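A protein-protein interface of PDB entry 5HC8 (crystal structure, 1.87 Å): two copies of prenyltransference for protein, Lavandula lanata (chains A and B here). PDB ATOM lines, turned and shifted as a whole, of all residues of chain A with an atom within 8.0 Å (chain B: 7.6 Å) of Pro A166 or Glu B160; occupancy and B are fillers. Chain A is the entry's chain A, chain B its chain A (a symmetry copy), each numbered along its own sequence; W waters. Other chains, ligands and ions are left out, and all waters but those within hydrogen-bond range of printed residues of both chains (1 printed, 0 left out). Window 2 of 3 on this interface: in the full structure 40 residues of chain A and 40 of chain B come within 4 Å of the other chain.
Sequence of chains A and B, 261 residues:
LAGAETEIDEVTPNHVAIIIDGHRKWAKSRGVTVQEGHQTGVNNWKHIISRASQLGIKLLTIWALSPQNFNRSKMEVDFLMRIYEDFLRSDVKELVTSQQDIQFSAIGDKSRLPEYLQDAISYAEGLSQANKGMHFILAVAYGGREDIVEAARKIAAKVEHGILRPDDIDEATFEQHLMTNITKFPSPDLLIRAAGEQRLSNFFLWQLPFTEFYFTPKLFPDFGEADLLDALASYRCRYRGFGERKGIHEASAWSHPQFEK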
ATOM      1  N   ILE A 155     -27.057  25.007  16.149  1.00  0.00           N
ATOM      2  CA  ILE A 155     -26.104  26.018  16.525  1.00  0.00           C
ATOM      3  C   ILE A 155     -25.661  26.762  15.264  1.00  0.00           C
ATOM      4  O   ILE A 155     -25.537  27.999  15.265  1.00  0.00           O
ATOM      5  CB  ILE A 155     -24.939  25.454  17.301  1.00  0.00           C
ATOM      6  CG1 ILE A 155     -25.395  25.187  18.727  1.00  0.00           C
ATOM      7  CG2 ILE A 155     -23.728  26.364  17.306  1.00  0.00           C
ATOM      8  CD1 ILE A 155     -24.545  24.152  19.420  1.00  0.00           C
ATOM      9  N   ALA A 156     -25.493  26.046  14.165  1.00  0.00           N
ATOM     10  CA  ALA A 156     -25.023  26.740  12.970  1.00  0.00           C
ATOM     11  C   ALA A 156     -26.159  27.703  12.457  1.00  0.00           C
ATOM     12  O   ALA A 156     -25.879  28.808  12.010  1.00  0.00           O
ATOM     13  CB  ALA A 156     -24.590  25.729  11.901  1.00  0.00           C
ATOM     14  N   VAL A 159     -25.898  30.852  14.315  1.00  0.00           N
ATOM     15  CA  VAL A 159     -24.695  31.578  13.907  1.00  0.00           C
ATOM     16  C   VAL A 159     -25.035  32.291  12.605  1.00  0.00           C
ATOM     17  O   VAL A 159     -24.732  33.463  12.473  1.00  0.00           O
ATOM     18  CB  VAL A 159     -23.439  30.674  13.728  1.00  0.00           C
ATOM     19  CG1 VAL A 159     -22.301  31.358  12.933  1.00  0.00           C
ATOM     20  CG2 VAL A 159     -22.853  30.289  15.087  1.00  0.00           C
ATOM     21  N   GLU A 160     -25.701  31.582  11.692  1.00  0.00           N
ATOM     22  CA  GLU A 160     -26.188  32.145  10.439  1.00  0.00           C
ATOM     23  C   GLU A 160     -27.102  33.365  10.674  1.00  0.00           C
ATOM     24  O   GLU A 160     -26.958  34.356   9.982  1.00  0.00           O
ATOM     25  CB  GLU A 160     -26.940  31.093   9.619  1.00  0.00           C
ATOM     26  CG  GLU A 160     -27.244  31.514   8.177  1.00  0.00           C
ATOM     27  CD  GLU A 160     -27.895  30.421   7.320  1.00  0.00           C
ATOM     28  OE1 GLU A 160     -28.960  29.881   7.703  1.00  0.00           O
ATOM     29  OE2 GLU A 160     -27.363  30.120   6.229  1.00  0.00           O
ATOM     30  N   GLY A 162     -27.081  35.350  13.328  1.00  0.00           N
ATOM     31  CA  GLY A 162     -26.468  36.356  14.148  1.00  0.00           C
ATOM     32  C   GLY A 162     -26.668  36.180  15.633  1.00  0.00           C
ATOM     33  O   GLY A 162     -26.094  36.942  16.392  1.00  0.00           O
ATOM     34  N   ILE A 163     -27.462  35.204  16.070  1.00  0.00           N
ATOM     35  CA  ILE A 163     -27.746  35.018  17.513  1.00  0.00           C
ATOM     36  C   ILE A 163     -26.510  34.573  18.324  1.00  0.00           C
ATOM     37  O   ILE A 163     -26.464  34.761  19.541  1.00  0.00           O
ATOM     38  CB  ILE A 163     -28.836  33.980  17.685  1.00  0.00           C
ATOM     39  CG1 ILE A 163     -30.128  34.491  17.029  1.00  0.00           C
ATOM     40  CG2 ILE A 163     -29.034  33.637  19.153  1.00  0.00           C
ATOM     41  CD1 ILE A 163     -30.870  33.443  16.210  1.00  0.00           C
ATOM     42  N   LEU A 164     -25.511  34.002  17.635  1.00  0.00           N
ATOM     43  CA  LEU A 164     -24.376  33.342  18.268  1.00  0.00           C
ATOM     44  C   LEU A 164     -23.135  33.561  17.429  1.00  0.00           C
ATOM     45  O   LEU A 164     -23.185  33.464  16.222  1.00  0.00           O
ATOM     46  CB  LEU A 164     -24.706  31.845  18.340  1.00  0.00           C
ATOM     47  CG  LEU A 164     -24.431  31.015  19.576  1.00  0.00           C
ATOM     48  CD1 LEU A 164     -25.076  31.603  20.801  1.00  0.00           C
ATOM     49  CD2 LEU A 164     -24.964  29.608  19.350  1.00  0.00           C
ATOM     50  N   ARG A 165     -22.014  33.834  18.054  1.00  0.00           N
ATOM     51  CA  ARG A 165     -20.734  33.872  17.348  1.00  0.00           C
ATOM     52  C   ARG A 165     -20.023  32.500  17.486  1.00  0.00           C
ATOM     53  O   ARG A 165     -20.253  31.777  18.444  1.00  0.00           O
ATOM     54  CB  ARG A 165     -19.817  34.950  17.953  1.00  0.00           C
ATOM     55  CG  ARG A 165     -19.548  36.161  17.052  1.00  0.00           C
ATOM     56  CD  ARG A 165     -19.435  37.475  17.818  1.00  0.00           C
ATOM     57  NE  ARG A 165     -18.547  37.437  18.992  1.00  0.00           N
ATOM     58  CZ  ARG A 165     -18.923  37.183  20.246  1.00  0.00           C
ATOM     59  NH1 ARG A 165     -20.193  36.905  20.531  1.00  0.00           N
ATOM     60  NH2 ARG A 165     -18.029  37.213  21.229  1.00  0.00           N
ATOM     61  N   PRO A 166     -19.143  32.156  16.551  1.00  0.00           N
ATOM     62  CA  PRO A 166     -18.457  30.877  16.720  1.00  0.00           C
ATOM     63  C   PRO A 166     -17.687  30.704  18.039  1.00  0.00           C
ATOM     64  O   PRO A 166     -17.788  29.638  18.677  1.00  0.00           O
ATOM     65  CB  PRO A 166     -17.532  30.838  15.510  1.00  0.00           C
ATOM     66  CG  PRO A 166     -18.377  31.453  14.454  1.00  0.00           C
ATOM     67  CD  PRO A 166     -19.088  32.600  15.154  1.00  0.00           C
ATOM     68  N   ASP A 167     -16.971  31.727  18.486  1.00  0.00           N
ATOM     69  CA  ASP A 167     -16.295  31.620  19.798  1.00  0.00           C
ATOM     70  C   ASP A 167     -17.218  31.600  21.027  1.00  0.00           C
ATOM     71  O   ASP A 167     -16.775  31.280  22.113  1.00  0.00           O
ATOM     72  CB  ASP A 167     -15.209  32.691  19.952  1.00  0.00           C
ATOM     73  CG  ASP A 167     -13.915  32.324  19.213  1.00  0.00           C
ATOM     74  OD1 ASP A 167     -13.940  31.421  18.338  1.00  0.00           O
ATOM     75  OD2 ASP A 167     -12.863  32.938  19.514  1.00  0.00           O
ATOM     76  N   ASP A 168     -18.498  31.868  20.866  1.00  0.00           N
ATOM     77  CA  ASP A 168     -19.441  31.650  21.947  1.00  0.00           C
ATOM     78  C   ASP A 168     -19.786  30.198  22.153  1.00  0.00           C
ATOM     79  O   ASP A 168     -20.454  29.871  23.117  1.00  0.00           O
ATOM     80  CB  ASP A 168     -20.767  32.382  21.710  1.00  0.00           C
ATOM     81  CG  ASP A 168     -20.600  33.908  21.444  1.00  0.00           C
ATOM     82  OD1 ASP A 168     -19.560  34.522  21.839  1.00  0.00           O
ATOM     83  OD2 ASP A 168     -21.566  34.458  20.832  1.00  0.00           O
ATOM     84  N   ILE A 169     -19.405  29.315  21.225  1.00  0.00           N
ATOM     85  CA  ILE A 169     -19.784  27.920  21.348  1.00  0.00           C
ATOM     86  C   ILE A 169     -18.888  27.215  22.404  1.00  0.00           C
ATOM     87  O   ILE A 169     -17.670  27.110  22.236  1.00  0.00           O
ATOM     88  CB  ILE A 169     -19.742  27.157  19.976  1.00  0.00           C
ATOM     89  CG1 ILE A 169     -20.666  27.831  18.965  1.00  0.00           C
ATOM     90  CG2 ILE A 169     -20.212  25.712  20.155  1.00  0.00           C
ATOM     91  CD1 ILE A 169     -20.257  27.556  17.545  1.00  0.00           C
ATOM     92  N   ASP A 170     -19.489  26.815  23.517  1.00  0.00           N
ATOM     93  CA  ASP A 170     -18.744  26.124  24.580  1.00  0.00           C
ATOM     94  C   ASP A 170     -19.494  24.878  24.922  1.00  0.00           C
ATOM     95  O   ASP A 170     -20.600  24.646  24.362  1.00  0.00           O
ATOM     96  CB  ASP A 170     -18.548  27.041  25.799  1.00  0.00           C
ATOM     97  CG  ASP A 170     -19.821  27.630  26.280  1.00  0.00           C
ATOM     98  OD1 ASP A 170     -20.895  27.168  25.885  1.00  0.00           O
ATOM     99  OD2 ASP A 170     -19.756  28.606  27.080  1.00  0.00           O
ATOM    100  N   THR A 173     -23.154  25.513  25.819  1.00  0.00           N
ATOM    101  CA  THR A 173     -24.023  25.873  24.687  1.00  0.00           C
ATOM    102  C   THR A 173     -24.358  24.635  23.845  1.00  0.00           C
ATOM    103  O   THR A 173     -25.484  24.388  23.443  1.00  0.00           O
ATOM    104  CB  THR A 173     -23.294  26.941  23.813  1.00  0.00           C
ATOM    105  OG1 THR A 173     -23.093  28.114  24.641  1.00  0.00           O
ATOM    106  CG2 THR A 173     -24.151  27.292  22.618  1.00  0.00           C
ATOM    107  N   VAL B 149     -16.531  20.212  20.632  1.00  0.00           N
ATOM    108  CA  VAL B 149     -16.836  21.666  20.701  1.00  0.00           C
ATOM    109  C   VAL B 149     -15.977  22.412  19.679  1.00  0.00           C
ATOM    110  O   VAL B 149     -16.476  23.257  18.960  1.00  0.00           O
ATOM    111  CB  VAL B 149     -16.589  22.224  22.120  1.00  0.00           C
ATOM    112  CG1 VAL B 149     -16.680  23.762  22.141  1.00  0.00           C
ATOM    113  CG2 VAL B 149     -17.579  21.660  23.130  1.00  0.00           C
ATOM    114  N   ALA B 152     -17.312  21.887  16.306  1.00  0.00           N
ATOM    115  CA  ALA B 152     -18.482  22.741  16.227  1.00  0.00           C
ATOM    116  C   ALA B 152     -18.104  24.241  15.947  1.00  0.00           C
ATOM    117  O   ALA B 152     -18.749  24.895  15.086  1.00  0.00           O
ATOM    118  CB  ALA B 152     -19.359  22.580  17.459  1.00  0.00           C
ATOM    119  N   ARG B 153     -17.034  24.705  16.579  1.00  0.00           N
ATOM    120  CA  ARG B 153     -16.594  26.078  16.427  1.00  0.00           C
ATOM    121  C   ARG B 153     -16.095  26.251  15.009  1.00  0.00           C
ATOM    122  O   ARG B 153     -16.484  27.203  14.343  1.00  0.00           O
ATOM    123  CB  ARG B 153     -15.476  26.441  17.379  1.00  0.00           C
ATOM    124  CG  ARG B 153     -15.881  26.557  18.827  1.00  0.00           C
ATOM    125  CD  ARG B 153     -14.768  27.153  19.669  1.00  0.00           C
ATOM    126  NE  ARG B 153     -15.129  27.111  21.086  1.00  0.00           N
ATOM    127  CZ  ARG B 153     -14.833  28.046  21.992  1.00  0.00           C
ATOM    128  NH1 ARG B 153     -14.173  29.143  21.632  1.00  0.00           N
ATOM    129  NH2 ARG B 153     -15.217  27.892  23.272  1.00  0.00           N
ATOM    130  N   LYS B 154     -15.225  25.336  14.552  1.00  0.00           N
ATOM    131  CA  LYS B 154     -14.678  25.401  13.154  1.00  0.00           C
ATOM    132  C   LYS B 154     -15.768  25.371  12.102  1.00  0.00           C
ATOM    133  O   LYS B 154     -15.690  26.094  11.079  1.00  0.00           O
ATOM    134  CB  LYS B 154     -13.673  24.272  12.858  1.00  0.00           C
ATOM    135  CG  LYS B 154     -12.342  24.289  13.535  1.00  0.00           C
ATOM    136  CD  LYS B 154     -11.620  22.970  13.191  1.00  0.00           C
ATOM    137  CE  LYS B 154     -10.103  22.981  13.348  1.00  0.00           C
ATOM    138  NZ  LYS B 154      -9.661  23.256  14.733  1.00  0.00           N
ATOM    139  N   ILE B 155     -16.796  24.559  12.290  1.00  0.00           N
ATOM    140  CA  ILE B 155     -17.909  24.482  11.380  1.00  0.00           C
ATOM    141  C   ILE B 155     -18.703  25.786  11.471  1.00  0.00           C
ATOM    142  O   ILE B 155     -19.134  26.342  10.446  1.00  0.00           O
ATOM    143  CB  ILE B 155     -18.769  23.266  11.622  1.00  0.00           C
ATOM    144  CG1 ILE B 155     -18.060  22.052  11.042  1.00  0.00           C
ATOM    145  CG2 ILE B 155     -20.157  23.388  11.027  1.00  0.00           C
ATOM    146  CD1 ILE B 155     -18.511  20.761  11.677  1.00  0.00           C
ATOM    147  N   ALA B 156     -18.841  26.330  12.668  1.00  0.00           N
ATOM    148  CA  ALA B 156     -19.639  27.548  12.771  1.00  0.00           C
ATOM    149  C   ALA B 156     -18.868  28.725  12.061  1.00  0.00           C
ATOM    150  O   ALA B 156     -19.480  29.556  11.402  1.00  0.00           O
ATOM    151  CB  ALA B 156     -19.951  27.860  14.240  1.00  0.00           C
ATOM    152  N   ALA B 157     -17.551  28.779  12.191  1.00  0.00           N
ATOM    153  CA  ALA B 157     -16.781  29.794  11.528  1.00  0.00           C
ATOM    154  C   ALA B 157     -16.974  29.723  10.027  1.00  0.00           C
ATOM    155  O   ALA B 157     -17.130  30.748   9.407  1.00  0.00           O
ATOM    156  CB  ALA B 157     -15.323  29.701  11.875  1.00  0.00           C
ATOM    157  N   LYS B 158     -17.003  28.509   9.466  1.00  0.00           N
ATOM    158  CA  LYS B 158     -17.275  28.312   8.040  1.00  0.00           C
ATOM    159  C   LYS B 158     -18.647  28.756   7.606  1.00  0.00           C
ATOM    160  O   LYS B 158     -18.778  29.231   6.463  1.00  0.00           O
ATOM    161  CB  LYS B 158     -17.082  26.837   7.609  1.00  0.00           C
ATOM    162  CG  LYS B 158     -15.629  26.407   7.567  1.00  0.00           C
ATOM    163  CD  LYS B 158     -15.466  25.124   6.752  1.00  0.00           C
ATOM    164  CE  LYS B 158     -14.036  24.626   6.911  1.00  0.00           C
ATOM    165  NZ  LYS B 158     -13.882  23.292   6.327  1.00  0.00           N
ATOM    166  N   VAL B 159     -19.646  28.589   8.482  1.00  0.00           N
ATOM    167  CA  VAL B 159     -21.039  28.975   8.256  1.00  0.00           C
ATOM    168  C   VAL B 159     -21.081  30.498   8.280  1.00  0.00           C
ATOM    169  O   VAL B 159     -21.687  31.088   7.405  1.00  0.00           O
ATOM    170  CB  VAL B 159     -22.038  28.379   9.291  1.00  0.00           C
ATOM    171  CG1 VAL B 159     -23.415  29.087   9.291  1.00  0.00           C
ATOM    172  CG2 VAL B 159     -22.305  26.902   8.996  1.00  0.00           C
ATOM    173  N   GLU B 160     -20.397  31.098   9.255  1.00  0.00           N
ATOM    174  CA  GLU B 160     -20.254  32.544   9.360  1.00  0.00           C
ATOM    175  C   GLU B 160     -19.654  33.157   8.079  1.00  0.00           C
ATOM    176  O   GLU B 160     -20.141  34.175   7.622  1.00  0.00           O
ATOM    177  CB  GLU B 160     -19.387  32.926  10.563  1.00  0.00           C
ATOM    178  CG  GLU B 160     -19.411  34.418  10.912  1.00  0.00           C
ATOM    179  CD  GLU B 160     -18.635  34.785  12.184  1.00  0.00           C
ATOM    180  OE1 GLU B 160     -17.424  34.474  12.286  1.00  0.00           O
ATOM    181  OE2 GLU B 160     -19.226  35.428  13.080  1.00  0.00           O
ATOM    182  N   HIS B 161     -18.606  32.545   7.528  1.00  0.00           N
ATOM    183  CA  HIS B 161     -17.989  33.000   6.292  1.00  0.00           C
ATOM    184  C   HIS B 161     -18.636  32.496   4.987  1.00  0.00           C
ATOM    185  O   HIS B 161     -18.085  32.703   3.946  1.00  0.00           O
ATOM    186  CB  HIS B 161     -16.503  32.656   6.281  1.00  0.00           C
ATOM    187  CG  HIS B 161     -15.713  33.413   7.294  1.00  0.00           C
ATOM    188  ND1 HIS B 161     -14.900  32.795   8.220  1.00  0.00           N
ATOM    189  CD2 HIS B 161     -15.623  34.742   7.539  1.00  0.00           C
ATOM    190  CE1 HIS B 161     -14.336  33.711   8.987  1.00  0.00           C
ATOM    191  NE2 HIS B 161     -14.753  34.900   8.590  1.00  0.00           N
ATOM    192  N   GLY B 162     -19.792  31.858   5.032  1.00  0.00           N
ATOM    193  CA  GLY B 162     -20.514  31.490   3.848  1.00  0.00           C
ATOM    194  C   GLY B 162     -20.064  30.206   3.197  1.00  0.00           C
ATOM    195  O   GLY B 162     -20.697  29.783   2.244  1.00  0.00           O
ATOM    196  N   ILE B 163     -18.995  29.574   3.678  1.00  0.00           N
ATOM    197  CA  ILE B 163     -18.468  28.341   3.046  1.00  0.00           C
ATOM    198  C   ILE B 163     -19.421  27.134   3.179  1.00  0.00           C
ATOM    199  O   ILE B 163     -19.337  26.186   2.396  1.00  0.00           O
ATOM    200  CB  ILE B 163     -17.138  27.978   3.675  1.00  0.00           C
ATOM    201  CG1 ILE B 163     -16.126  29.100   3.397  1.00  0.00           C
ATOM    202  CG2 ILE B 163     -16.650  26.628   3.174  1.00  0.00           C
ATOM    203  CD1 ILE B 163     -15.270  29.480   4.598  1.00  0.00           C
ATOM    204  N   LEU B 164     -20.332  27.191   4.162  1.00  0.00           N
ATOM    205  CA  LEU B 164     -21.160  26.058   4.553  1.00  0.00           C
ATOM    206  C   LEU B 164     -22.524  26.555   4.983  1.00  0.00           C
ATOM    207  O   LEU B 164     -22.626  27.539   5.683  1.00  0.00           O
ATOM    208  CB  LEU B 164     -20.456  25.369   5.730  1.00  0.00           C
ATOM    209  CG  LEU B 164     -20.332  23.863   5.829  1.00  0.00           C
ATOM    210  CD1 LEU B 164     -19.686  23.272   4.604  1.00  0.00           C
ATOM    211  CD2 LEU B 164     -19.498  23.519   7.055  1.00  0.00           C
ATOM    212  N   PRO B 166     -26.115  25.619   7.198  1.00  0.00           N
ATOM    213  CA  PRO B 166     -26.425  24.696   8.288  1.00  0.00           C
ATOM    214  C   PRO B 166     -26.927  23.307   7.860  1.00  0.00           C
ATOM    215  O   PRO B 166     -26.469  22.289   8.414  1.00  0.00           O
ATOM    216  CB  PRO B 166     -27.474  25.463   9.081  1.00  0.00           C
ATOM    217  CG  PRO B 166     -26.974  26.859   8.988  1.00  0.00           C
ATOM    218  CD  PRO B 166     -26.482  26.994   7.556  1.00  0.00           C
HETATM  219  O   HOH W   1     -16.795  30.337  24.995  1.00  0.00           O
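O of Asp A167 is in hydrogen-bond range of NH1 of Arg B153. O of Ile A169 lies within hydrogen-bond range of NH2 of Arg B153 (2.8 Å).
The side-chain carboxylate (OD1) of Asp A170 is in hydrogen-bond range of the side-chain hydroxyl (OG1) of Thr A173 (2.7 Å). The backbone carbonyl oxygen (O) of Ala B157 lies within hydrogen-bond range of a ring nitrogen (ND1) of His B161 (3.3 Å).
Among the printed residues, pairs that only touch across the chains: Ala A156 with Val B159 (3.7 Å), Ala A156 with Pro B166 (3.7 Å), Val A159 with Ala B156 (3.7 Å), Glu A160 with Pro B166 (3.5 Å), Pro A166 with Arg B153 (3.6 Å), Pro A166 with Ala B156 (3.7 Å), Pro A166 with Ala B157 (3.6 Å), Pro A166 with Glu B160 (3.5 Å), Ile A169 with Val B149 (3.5 Å), Ile A169 with Ala B152 (3.9 Å), Ile A169 with Ala B156 (3.3 Å) and Asp A170 with Val B149 (3.97 Å).
Of the printed residues of chain B, Glu A160 touches Pro B166 (3.5 Å). Of the printed residues of chain B, Asp A170 touches Val B149. Of the printed residues of chain A, Ala B152 touches Ile A169 (3.9 Å). Of the printed residues of chain A, Ala B156 touches Val A159, Pro A166 and Ile A169. Of chain A, only Pro A166 (3.5 Å) comes within 4 Å of Glu B160. Printed residues of chain A within 4 Å of Pro B166: Ala A156 and Glu A160. The nearest residue of chain B that does not touch Pro A166 is Lys B158 (6.0 Å).
Of the 15 printed residues of chain B, 8 touch a printed residue of chain A. Hydrophobic or aromatic side chains of chain B within 4 Å of the printed part of chain A: Val B149, Ala B156, Val B159 and Pro B166. Among the printed residues, no Asp or Glu carboxylate lies within 4 Å of a Lys or Arg side-chain nitrogen of the other chain.
Ala A156 touches Val B159, and with the chains exchanged Val A159 touches Ala B156. Ala A156 touches Pro B166, and with the chains exchanged Pro A166 touches Ala B156. Glu A160 touches Pro B166, and with the chains exchanged Pro A166 touches Glu B160. Positions printed for both chains: 155, 156, 159, 160, 162, 163, 164 and 166. Of the 14 pairs that touch across the chains among the printed residues, 6 have their exchanged pair printed and touching as well.
Water W1 lies within hydrogen-bond range of O of Asp A167 and NH2 of Arg B153.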
